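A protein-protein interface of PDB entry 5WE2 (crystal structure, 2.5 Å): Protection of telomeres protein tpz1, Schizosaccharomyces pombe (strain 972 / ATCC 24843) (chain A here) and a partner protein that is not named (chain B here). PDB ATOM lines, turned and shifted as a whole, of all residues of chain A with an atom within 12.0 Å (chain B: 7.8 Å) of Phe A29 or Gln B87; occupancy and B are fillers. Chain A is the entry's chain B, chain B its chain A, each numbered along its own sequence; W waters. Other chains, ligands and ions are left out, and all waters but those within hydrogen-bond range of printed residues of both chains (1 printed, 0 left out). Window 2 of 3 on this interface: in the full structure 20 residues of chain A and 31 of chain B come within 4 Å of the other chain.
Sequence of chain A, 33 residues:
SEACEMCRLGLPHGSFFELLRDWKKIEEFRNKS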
ATOM      1  N   LEU A  20       7.257 -16.826  12.838  1.00  0.00           N
ATOM      2  CA  LEU A  20       7.892 -15.547  13.145  1.00  0.00           C
ATOM      3  C   LEU A  20       7.152 -14.770  14.237  1.00  0.00           C
ATOM      4  O   LEU A  20       7.754 -14.249  15.207  1.00  0.00           O
ATOM      5  CB  LEU A  20       7.974 -14.702  11.880  1.00  0.00           C
ATOM      6  CG  LEU A  20       8.405 -13.253  12.067  1.00  0.00           C
ATOM      7  CD1 LEU A  20       9.895 -13.222  12.424  1.00  0.00           C
ATOM      8  CD2 LEU A  20       8.043 -12.394  10.808  1.00  0.00           C
ATOM      9  N   ARG A  21       5.835 -14.690  14.097  1.00  0.00           N
ATOM     10  CA  ARG A  21       5.080 -13.882  15.058  1.00  0.00           C
ATOM     11  C   ARG A  21       5.048 -14.496  16.459  1.00  0.00           C
ATOM     12  O   ARG A  21       5.182 -13.789  17.470  1.00  0.00           O
ATOM     13  CB  ARG A  21       3.655 -13.663  14.557  1.00  0.00           C
ATOM     14  CG  ARG A  21       3.593 -12.707  13.397  1.00  0.00           C
ATOM     15  CD  ARG A  21       2.263 -12.011  13.365  1.00  0.00           C
ATOM     16  NE  ARG A  21       1.202 -12.994  13.217  1.00  0.00           N
ATOM     17  CZ  ARG A  21      -0.054 -12.714  12.883  1.00  0.00           C
ATOM     18  NH1 ARG A  21      -0.434 -11.455  12.638  1.00  0.00           N
ATOM     19  NH2 ARG A  21      -0.926 -13.711  12.785  1.00  0.00           N
ATOM     20  N   ASP A  22       4.856 -15.812  16.511  1.00  0.00           N
ATOM     21  CA  ASP A  22       4.878 -16.530  17.786  1.00  0.00           C
ATOM     22  C   ASP A  22       6.248 -16.424  18.475  1.00  0.00           C
ATOM     23  O   ASP A  22       6.353 -16.120  19.663  1.00  0.00           O
ATOM     24  CB  ASP A  22       4.490 -17.977  17.543  1.00  0.00           C
ATOM     25  CG  ASP A  22       2.997 -18.129  17.259  1.00  0.00           C
ATOM     26  OD1 ASP A  22       2.255 -17.122  17.474  1.00  0.00           O
ATOM     27  OD2 ASP A  22       2.571 -19.246  16.851  1.00  0.00           O
ATOM     28  N   TRP A  23       7.297 -16.609  17.690  1.00  0.00           N
ATOM     29  CA  TRP A  23       8.660 -16.426  18.159  1.00  0.00           C
ATOM     30  C   TRP A  23       8.891 -15.066  18.816  1.00  0.00           C
ATOM     31  O   TRP A  23       9.453 -14.990  19.937  1.00  0.00           O
ATOM     32  CB  TRP A  23       9.633 -16.604  16.999  1.00  0.00           C
ATOM     33  CG  TRP A  23      10.993 -16.951  17.456  1.00  0.00           C
ATOM     34  CD1 TRP A  23      11.943 -16.102  17.954  1.00  0.00           C
ATOM     35  CD2 TRP A  23      11.564 -18.258  17.487  1.00  0.00           C
ATOM     36  NE1 TRP A  23      13.081 -16.801  18.268  1.00  0.00           N
ATOM     37  CE2 TRP A  23      12.871 -18.130  17.996  1.00  0.00           C
ATOM     38  CE3 TRP A  23      11.104 -19.520  17.112  1.00  0.00           C
ATOM     39  CZ2 TRP A  23      13.718 -19.228  18.153  1.00  0.00           C
ATOM     40  CZ3 TRP A  23      11.950 -20.607  17.264  1.00  0.00           C
ATOM     41  CH2 TRP A  23      13.235 -20.456  17.783  1.00  0.00           C
ATOM     42  N   LYS A  24       8.456 -13.996  18.141  1.00  0.00           N
ATOM     43  CA  LYS A  24       8.546 -12.639  18.727  1.00  0.00           C
ATOM     44  C   LYS A  24       7.696 -12.432  19.990  1.00  0.00           C
ATOM     45  O   LYS A  24       8.111 -11.745  20.919  1.00  0.00           O
ATOM     46  CB  LYS A  24       8.157 -11.585  17.677  1.00  0.00           C
ATOM     47  CG  LYS A  24       8.949 -11.736  16.352  1.00  0.00           C
ATOM     48  CD  LYS A  24       9.212 -10.405  15.684  1.00  0.00           C
ATOM     49  CE  LYS A  24       7.925  -9.591  15.480  1.00  0.00           C
ATOM     50  NZ  LYS A  24       8.200  -8.125  15.614  1.00  0.00           N
ATOM     51  N   LYS A  25       6.489 -12.980  20.007  1.00  0.00           N
ATOM     52  CA  LYS A  25       5.682 -12.987  21.220  1.00  0.00           C
ATOM     53  C   LYS A  25       6.464 -13.587  22.418  1.00  0.00           C
ATOM     54  O   LYS A  25       6.552 -12.997  23.509  1.00  0.00           O
ATOM     55  CB  LYS A  25       4.413 -13.802  20.993  1.00  0.00           C
ATOM     56  CG  LYS A  25       3.272 -13.109  20.289  1.00  0.00           C
ATOM     57  CD  LYS A  25       2.193 -14.153  20.003  1.00  0.00           C
ATOM     58  CE  LYS A  25       0.811 -13.577  19.756  1.00  0.00           C
ATOM     59  NZ  LYS A  25      -0.235 -14.673  19.742  1.00  0.00           N
ATOM     60  N   ILE A  26       7.046 -14.759  22.202  1.00  0.00           N
ATOM     61  CA  ILE A  26       7.788 -15.393  23.276  1.00  0.00           C
ATOM     62  C   ILE A  26       8.983 -14.556  23.703  1.00  0.00           C
ATOM     63  O   ILE A  26       9.233 -14.360  24.900  1.00  0.00           O
ATOM     64  CB  ILE A  26       8.287 -16.781  22.871  1.00  0.00           C
ATOM     65  CG1 ILE A  26       7.125 -17.732  22.566  1.00  0.00           C
ATOM     66  CG2 ILE A  26       9.196 -17.337  23.927  1.00  0.00           C
ATOM     67  CD1 ILE A  26       7.589 -18.933  21.698  1.00  0.00           C
ATOM     68  N   GLU A  27       9.735 -14.064  22.727  1.00  0.00           N
ATOM     69  CA  GLU A  27      10.936 -13.310  23.053  1.00  0.00           C
ATOM     70  C   GLU A  27      10.627 -12.005  23.799  1.00  0.00           C
ATOM     71  O   GLU A  27      11.350 -11.620  24.718  1.00  0.00           O
ATOM     72  CB  GLU A  27      11.726 -13.026  21.786  1.00  0.00           C
ATOM     73  CG  GLU A  27      13.086 -12.429  22.043  1.00  0.00           C
ATOM     74  CD  GLU A  27      13.960 -12.447  20.801  1.00  0.00           C
ATOM     75  OE1 GLU A  27      13.435 -12.109  19.711  1.00  0.00           O
ATOM     76  OE2 GLU A  27      15.164 -12.798  20.921  1.00  0.00           O
ATOM     77  N   GLU A  28       9.550 -11.329  23.411  1.00  0.00           N
ATOM     78  CA  GLU A  28       9.144 -10.106  24.088  1.00  0.00           C
ATOM     79  C   GLU A  28       8.666 -10.392  25.498  1.00  0.00           C
ATOM     80  O   GLU A  28       8.990  -9.669  26.439  1.00  0.00           O
ATOM     81  CB  GLU A  28       8.057  -9.389  23.286  1.00  0.00           C
ATOM     82  CG  GLU A  28       8.626  -8.657  22.066  1.00  0.00           C
ATOM     83  CD  GLU A  28       7.555  -8.024  21.187  1.00  0.00           C
ATOM     84  OE1 GLU A  28       6.540  -7.545  21.739  1.00  0.00           O
ATOM     85  OE2 GLU A  28       7.739  -7.985  19.946  1.00  0.00           O
ATOM     86  N   PHE A  29       7.898 -11.461  25.648  1.00  0.00           N
ATOM     87  CA  PHE A  29       7.476 -11.885  26.966  1.00  0.00           C
ATOM     88  C   PHE A  29       8.660 -12.104  27.910  1.00  0.00           C
ATOM     89  O   PHE A  29       8.550 -11.849  29.099  1.00  0.00           O
ATOM     90  CB  PHE A  29       6.655 -13.153  26.853  1.00  0.00           C
ATOM     91  CG  PHE A  29       6.190 -13.694  28.166  1.00  0.00           C
ATOM     92  CD1 PHE A  29       5.091 -13.143  28.807  1.00  0.00           C
ATOM     93  CD2 PHE A  29       6.824 -14.793  28.740  1.00  0.00           C
ATOM     94  CE1 PHE A  29       4.638 -13.673  30.022  1.00  0.00           C
ATOM     95  CE2 PHE A  29       6.385 -15.329  29.954  1.00  0.00           C
ATOM     96  CZ  PHE A  29       5.297 -14.769  30.604  1.00  0.00           C
ATOM     97  N   ARG A  30       9.795 -12.550  27.385  1.00  0.00           N
ATOM     98  CA  ARG A  30      10.902 -12.930  28.262  1.00  0.00           C
ATOM     99  C   ARG A  30      11.884 -11.784  28.547  1.00  0.00           C
ATOM    100  O   ARG A  30      12.986 -12.021  29.030  1.00  0.00           O
ATOM    101  CB  ARG A  30      11.645 -14.151  27.691  1.00  0.00           C
ATOM    102  CG  ARG A  30      10.869 -15.425  27.927  1.00  0.00           C
ATOM    103  CD  ARG A  30      11.511 -16.702  27.401  1.00  0.00           C
ATOM    104  NE  ARG A  30      10.517 -17.771  27.483  1.00  0.00           N
ATOM    105  CZ  ARG A  30      10.632 -18.965  26.916  1.00  0.00           C
ATOM    106  NH1 ARG A  30      11.713 -19.275  26.208  1.00  0.00           N
ATOM    107  NH2 ARG A  30       9.648 -19.841  27.034  1.00  0.00           N
ATOM    108  N   ASN A  31      11.470 -10.549  28.261  1.00  0.00           N
ATOM    109  CA  ASN A  31      12.055  -9.363  28.907  1.00  0.00           C
ATOM    110  C   ASN A  31      11.107  -8.868  29.988  1.00  0.00           C
ATOM    111  O   ASN A  31      11.301  -9.085  31.198  1.00  0.00           O
ATOM    112  CB  ASN A  31      12.294  -8.258  27.903  1.00  0.00           C
ATOM    113  CG  ASN A  31      12.763  -8.790  26.584  1.00  0.00           C
ATOM    114  OD1 ASN A  31      13.313  -9.889  26.516  1.00  0.00           O
ATOM    115  ND2 ASN A  31      12.519  -8.033  25.511  1.00  0.00           N
ATOM    116  N   LYS A  32      10.061  -8.200  29.517  1.00  0.00           N
ATOM    117  CA  LYS A  32       8.925  -7.857  30.352  1.00  0.00           C
ATOM    118  C   LYS A  32       7.664  -8.029  29.516  1.00  0.00           C
ATOM    119  O   LYS A  32       7.734  -8.043  28.286  1.00  0.00           O
ATOM    120  CB  LYS A  32       9.048  -6.426  30.895  1.00  0.00           C
ATOM    121  CG  LYS A  32       9.871  -6.315  32.184  1.00  0.00           C
ATOM    122  CD  LYS A  32       9.332  -5.209  33.086  1.00  0.00           C
ATOM    123  CE  LYS A  32       8.595  -5.798  34.290  1.00  0.00           C
ATOM    124  NZ  LYS A  32       8.266  -4.786  35.331  1.00  0.00           N
ATOM    125  N   TYR B  63      11.938 -23.894  22.568  1.00  0.00           N
ATOM    126  CA  TYR B  63      11.954 -22.459  22.952  1.00  0.00           C
ATOM    127  C   TYR B  63      10.685 -22.041  23.708  1.00  0.00           C
ATOM    128  O   TYR B  63      10.725 -21.401  24.763  1.00  0.00           O
ATOM    129  CB  TYR B  63      12.131 -21.591  21.702  1.00  0.00           C
ATOM    130  CG  TYR B  63      12.282 -20.099  21.949  1.00  0.00           C
ATOM    131  CD1 TYR B  63      13.138 -19.624  22.931  1.00  0.00           C
ATOM    132  CD2 TYR B  63      11.577 -19.162  21.180  1.00  0.00           C
ATOM    133  CE1 TYR B  63      13.282 -18.274  23.162  1.00  0.00           C
ATOM    134  CE2 TYR B  63      11.719 -17.805  21.395  1.00  0.00           C
ATOM    135  CZ  TYR B  63      12.570 -17.367  22.385  1.00  0.00           C
ATOM    136  OH  TYR B  63      12.720 -16.024  22.636  1.00  0.00           O
ATOM    137  N   CYS B  64       9.552 -22.433  23.149  1.00  0.00           N
ATOM    138  CA  CYS B  64       8.243 -22.063  23.644  1.00  0.00           C
ATOM    139  C   CYS B  64       7.979 -22.589  25.046  1.00  0.00           C
ATOM    140  O   CYS B  64       7.599 -21.844  25.925  1.00  0.00           O
ATOM    141  CB  CYS B  64       7.168 -22.568  22.687  1.00  0.00           C
ATOM    142  SG  CYS B  64       5.506 -22.166  23.238  1.00  0.00           S
ATOM    143  N   ASN B  66      10.289 -23.735  26.988  1.00  0.00           N
ATOM    144  CA  ASN B  66      11.494 -23.552  27.780  1.00  0.00           C
ATOM    145  C   ASN B  66      12.056 -24.879  28.333  1.00  0.00           C
ATOM    146  O   ASN B  66      12.368 -24.982  29.501  1.00  0.00           O
ATOM    147  CB  ASN B  66      11.213 -22.596  28.935  1.00  0.00           C
ATOM    148  CG  ASN B  66      12.476 -21.964  29.475  1.00  0.00           C
ATOM    149  OD1 ASN B  66      13.395 -21.629  28.711  1.00  0.00           O
ATOM    150  ND2 ASN B  66      12.556 -21.841  30.795  1.00  0.00           N
ATOM    151  N   SER B  86       9.836 -19.236  36.932  1.00  0.00           N
ATOM    152  CA  SER B  86       8.933 -20.018  36.094  1.00  0.00           C
ATOM    153  C   SER B  86       7.984 -19.100  35.303  1.00  0.00           C
ATOM    154  O   SER B  86       6.942 -19.525  34.789  1.00  0.00           O
ATOM    155  CB  SER B  86       8.155 -21.017  36.954  1.00  0.00           C
ATOM    156  OG  SER B  86       9.048 -21.813  37.725  1.00  0.00           O
ATOM    157  N   GLN B  87       8.379 -17.836  35.194  1.00  0.00           N
ATOM    158  CA  GLN B  87       7.613 -16.827  34.486  1.00  0.00           C
ATOM    159  C   GLN B  87       8.030 -16.814  33.017  1.00  0.00           C
ATOM    160  O   GLN B  87       8.098 -15.757  32.393  1.00  0.00           O
ATOM    161  CB  GLN B  87       7.843 -15.443  35.116  1.00  0.00           C
ATOM    162  CG  GLN B  87       7.964 -15.423  36.657  1.00  0.00           C
ATOM    163  CD  GLN B  87       9.299 -15.955  37.182  1.00  0.00           C
ATOM    164  OE1 GLN B  87      10.147 -16.420  36.411  1.00  0.00           O
ATOM    165  NE2 GLN B  87       9.477 -15.912  38.502  1.00  0.00           N
ATOM    166  N   GLN B  88       8.329 -17.991  32.477  1.00  0.00           N
ATOM    167  CA  GLN B  88       9.002 -18.085  31.192  1.00  0.00           C
ATOM    168  C   GLN B  88       8.065 -18.524  30.071  1.00  0.00           C
ATOM    169  O   GLN B  88       8.191 -18.053  28.933  1.00  0.00           O
ATOM    170  CB  GLN B  88      10.206 -19.032  31.291  1.00  0.00           C
ATOM    171  CG  GLN B  88      11.402 -18.432  32.027  1.00  0.00           C
ATOM    172  CD  GLN B  88      11.725 -17.016  31.525  1.00  0.00           C
ATOM    173  OE1 GLN B  88      12.298 -16.841  30.447  1.00  0.00           O
ATOM    174  NE2 GLN B  88      11.332 -16.002  32.297  1.00  0.00           N
ATOM    175  N   ILE B  89       7.122 -19.408  30.387  1.00  0.00           N
ATOM    176  CA  ILE B  89       6.149 -19.853  29.399  1.00  0.00           C
ATOM    177  C   ILE B  89       5.015 -18.838  29.244  1.00  0.00           C
ATOM    178  O   ILE B  89       4.374 -18.469  30.222  1.00  0.00           O
ATOM    179  CB  ILE B  89       5.558 -21.218  29.756  1.00  0.00           C
ATOM    180  CG1 ILE B  89       6.672 -22.272  29.819  1.00  0.00           C
ATOM    181  CG2 ILE B  89       4.509 -21.604  28.722  1.00  0.00           C
ATOM    182  CD1 ILE B  89       6.211 -23.693  30.208  1.00  0.00           C
ATOM    183  N   LEU B  90       4.791 -18.361  28.022  1.00  0.00           N
ATOM    184  CA  LEU B  90       3.686 -17.429  27.773  1.00  0.00           C
ATOM    185  C   LEU B  90       2.410 -18.226  27.503  1.00  0.00           C
ATOM    186  O   LEU B  90       2.196 -18.713  26.387  1.00  0.00           O
ATOM    187  CB  LEU B  90       3.993 -16.491  26.600  1.00  0.00           C
ATOM    188  CG  LEU B  90       2.842 -15.588  26.077  1.00  0.00           C
ATOM    189  CD1 LEU B  90       2.288 -14.629  27.141  1.00  0.00           C
ATOM    190  CD2 LEU B  90       3.270 -14.794  24.840  1.00  0.00           C
ATOM    191  N   TRP B  91       1.583 -18.392  28.530  1.00  0.00           N
ATOM    192  CA  TRP B  91       0.324 -19.092  28.371  1.00  0.00           C
ATOM    193  C   TRP B  91      -0.703 -18.150  27.749  1.00  0.00           C
ATOM    194  O   TRP B  91      -1.553 -17.606  28.434  1.00  0.00           O
ATOM    195  CB  TRP B  91      -0.173 -19.648  29.717  1.00  0.00           C
ATOM    196  CG  TRP B  91       0.704 -20.728  30.224  1.00  0.00           C
ATOM    197  CD1 TRP B  91       1.679 -20.627  31.197  1.00  0.00           C
ATOM    198  CD2 TRP B  91       0.738 -22.089  29.758  1.00  0.00           C
ATOM    199  NE1 TRP B  91       2.294 -21.849  31.356  1.00  0.00           N
ATOM    200  CE2 TRP B  91       1.747 -22.754  30.483  1.00  0.00           C
ATOM    201  CE3 TRP B  91       0.016 -22.802  28.796  1.00  0.00           C
ATOM    202  CZ2 TRP B  91       2.049 -24.092  30.273  1.00  0.00           C
ATOM    203  CZ3 TRP B  91       0.316 -24.139  28.593  1.00  0.00           C
ATOM    204  CH2 TRP B  91       1.324 -24.769  29.322  1.00  0.00           C
ATOM    205  N   GLU B  92      -0.602 -17.941  26.446  1.00  0.00           N
ATOM    206  CA  GLU B  92      -1.566 -17.128  25.721  1.00  0.00           C
ATOM    207  C   GLU B  92      -2.252 -18.059  24.730  1.00  0.00           C
ATOM    208  O   GLU B  92      -1.597 -18.856  24.051  1.00  0.00           O
ATOM    209  CB  GLU B  92      -0.877 -15.943  25.035  1.00  0.00           C
ATOM    210  CG  GLU B  92      -1.781 -14.996  24.267  1.00  0.00           C
ATOM    211  CD  GLU B  92      -2.014 -15.431  22.813  1.00  0.00           C
ATOM    212  OE1 GLU B  92      -1.018 -15.613  22.068  1.00  0.00           O
ATOM    213  OE2 GLU B  92      -3.203 -15.592  22.419  1.00  0.00           O
ATOM    214  N   LEU B  95      -0.968 -18.398  20.880  1.00  0.00           N
ATOM    215  CA  LEU B  95       0.353 -19.007  20.930  1.00  0.00           C
ATOM    216  C   LEU B  95       0.290 -20.512  21.297  1.00  0.00           C
ATOM    217  O   LEU B  95       0.918 -21.364  20.645  1.00  0.00           O
ATOM    218  CB  LEU B  95       1.236 -18.278  21.938  1.00  0.00           C
ATOM    219  CG  LEU B  95       2.630 -18.904  22.082  1.00  0.00           C
ATOM    220  CD1 LEU B  95       3.353 -18.741  20.765  1.00  0.00           C
ATOM    221  CD2 LEU B  95       3.430 -18.262  23.177  1.00  0.00           C
HETATM  222  O   HOH W   1      13.948 -21.910  26.315  1.00  0.00           O
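The backbone carbonyl oxygen (O) of Tyr B63 sits at hydrogen-bond distance from the guanidinium group (NH1) of Arg A30.
NH2 of Arg A30 sits at hydrogen-bond distance from O of Cys B64, at 3.1 Å.
The backbone carbonyl oxygen of Gln B88 lies within hydrogen-bond range of the guanidinium group of Arg A30 (2.8 Å).
OE1 of Glu B92 lies within salt-bridge range of NZ of Lys A25 (2.6 Å).
Water W1 lies within hydrogen-bond range of the side-chain amide oxygen (OD1) of Asn B66 (2.5 Å) and the guanidinium group (NH1) of Arg A30 (3.5 Å).
Among the printed residues, pairs that only touch across the chains: Phe A29 with Gln B87 (3.0 Å), Glu A27 with Tyr B63 (3.3 Å), Phe A29 with Gln B88 (3.4 Å), Asp A22 with Leu B95 (3.5 Å), Trp A23 with Tyr B63 (3.6 Å), Phe A29 with Leu B90 (3.6 Å), Ile A26 with Tyr B63 (3.6 Å), Arg A30 with Asn B66 (3.7 Å), Phe A29 with Ile B89 (3.7 Å), Ile A26 with Cys B64 (3.7 Å), Ile A26 with Leu B95 (3.8 Å), Lys A25 with Leu B95 (3.96 Å) and Lys A25 with Leu B90 (3.97 Å).
The side-chain carboxylate (OE1) of Glu B92 lies within hydrogen-bond range of the backbone NH (N) of Leu B95 (3.0 Å).
The backbone carbonyl oxygen of Glu A27 lies close to the side-chain amide oxygen of Asn A31 (3.2 Å).
Hydrophobic or aromatic side chains of chain A that line the printed part of chain B: Trp A23, Ile A26 and Phe A29.
Hydrophobic or aromatic side chains of chain B within 4 Å of the printed part of chain A: Tyr B63, Leu B90 and Leu B95.
Among the printed residues, 17 pairs touch across the chains.
Of the printed residues of chain B, Asp A22 touches Leu B95.
Printed residues of chain B within 4 Å of Lys A25: Leu B90, Glu B92 and Leu B95.
Printed residues of chain B within 4 Å of Ile A26: Tyr B63, Cys B64 and Leu B95.
Printed residues of chain B within 4 Å of Glu A27: Tyr B63.
Of chain B, only Gln B87 (3.0 Å), Gln B88 (3.4 Å), Ile B89 (3.7 Å) and Leu B90 (3.6 Å) come within 4 Å of Phe A29.
No residue of chain A comes within 4 Å of Ser B86.
Leu B90 touches just these residues of chain A: Lys A25 and Phe A29.
The nearest residue of chain A that does not touch Gln B87 is Arg A30 (5.3 Å).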
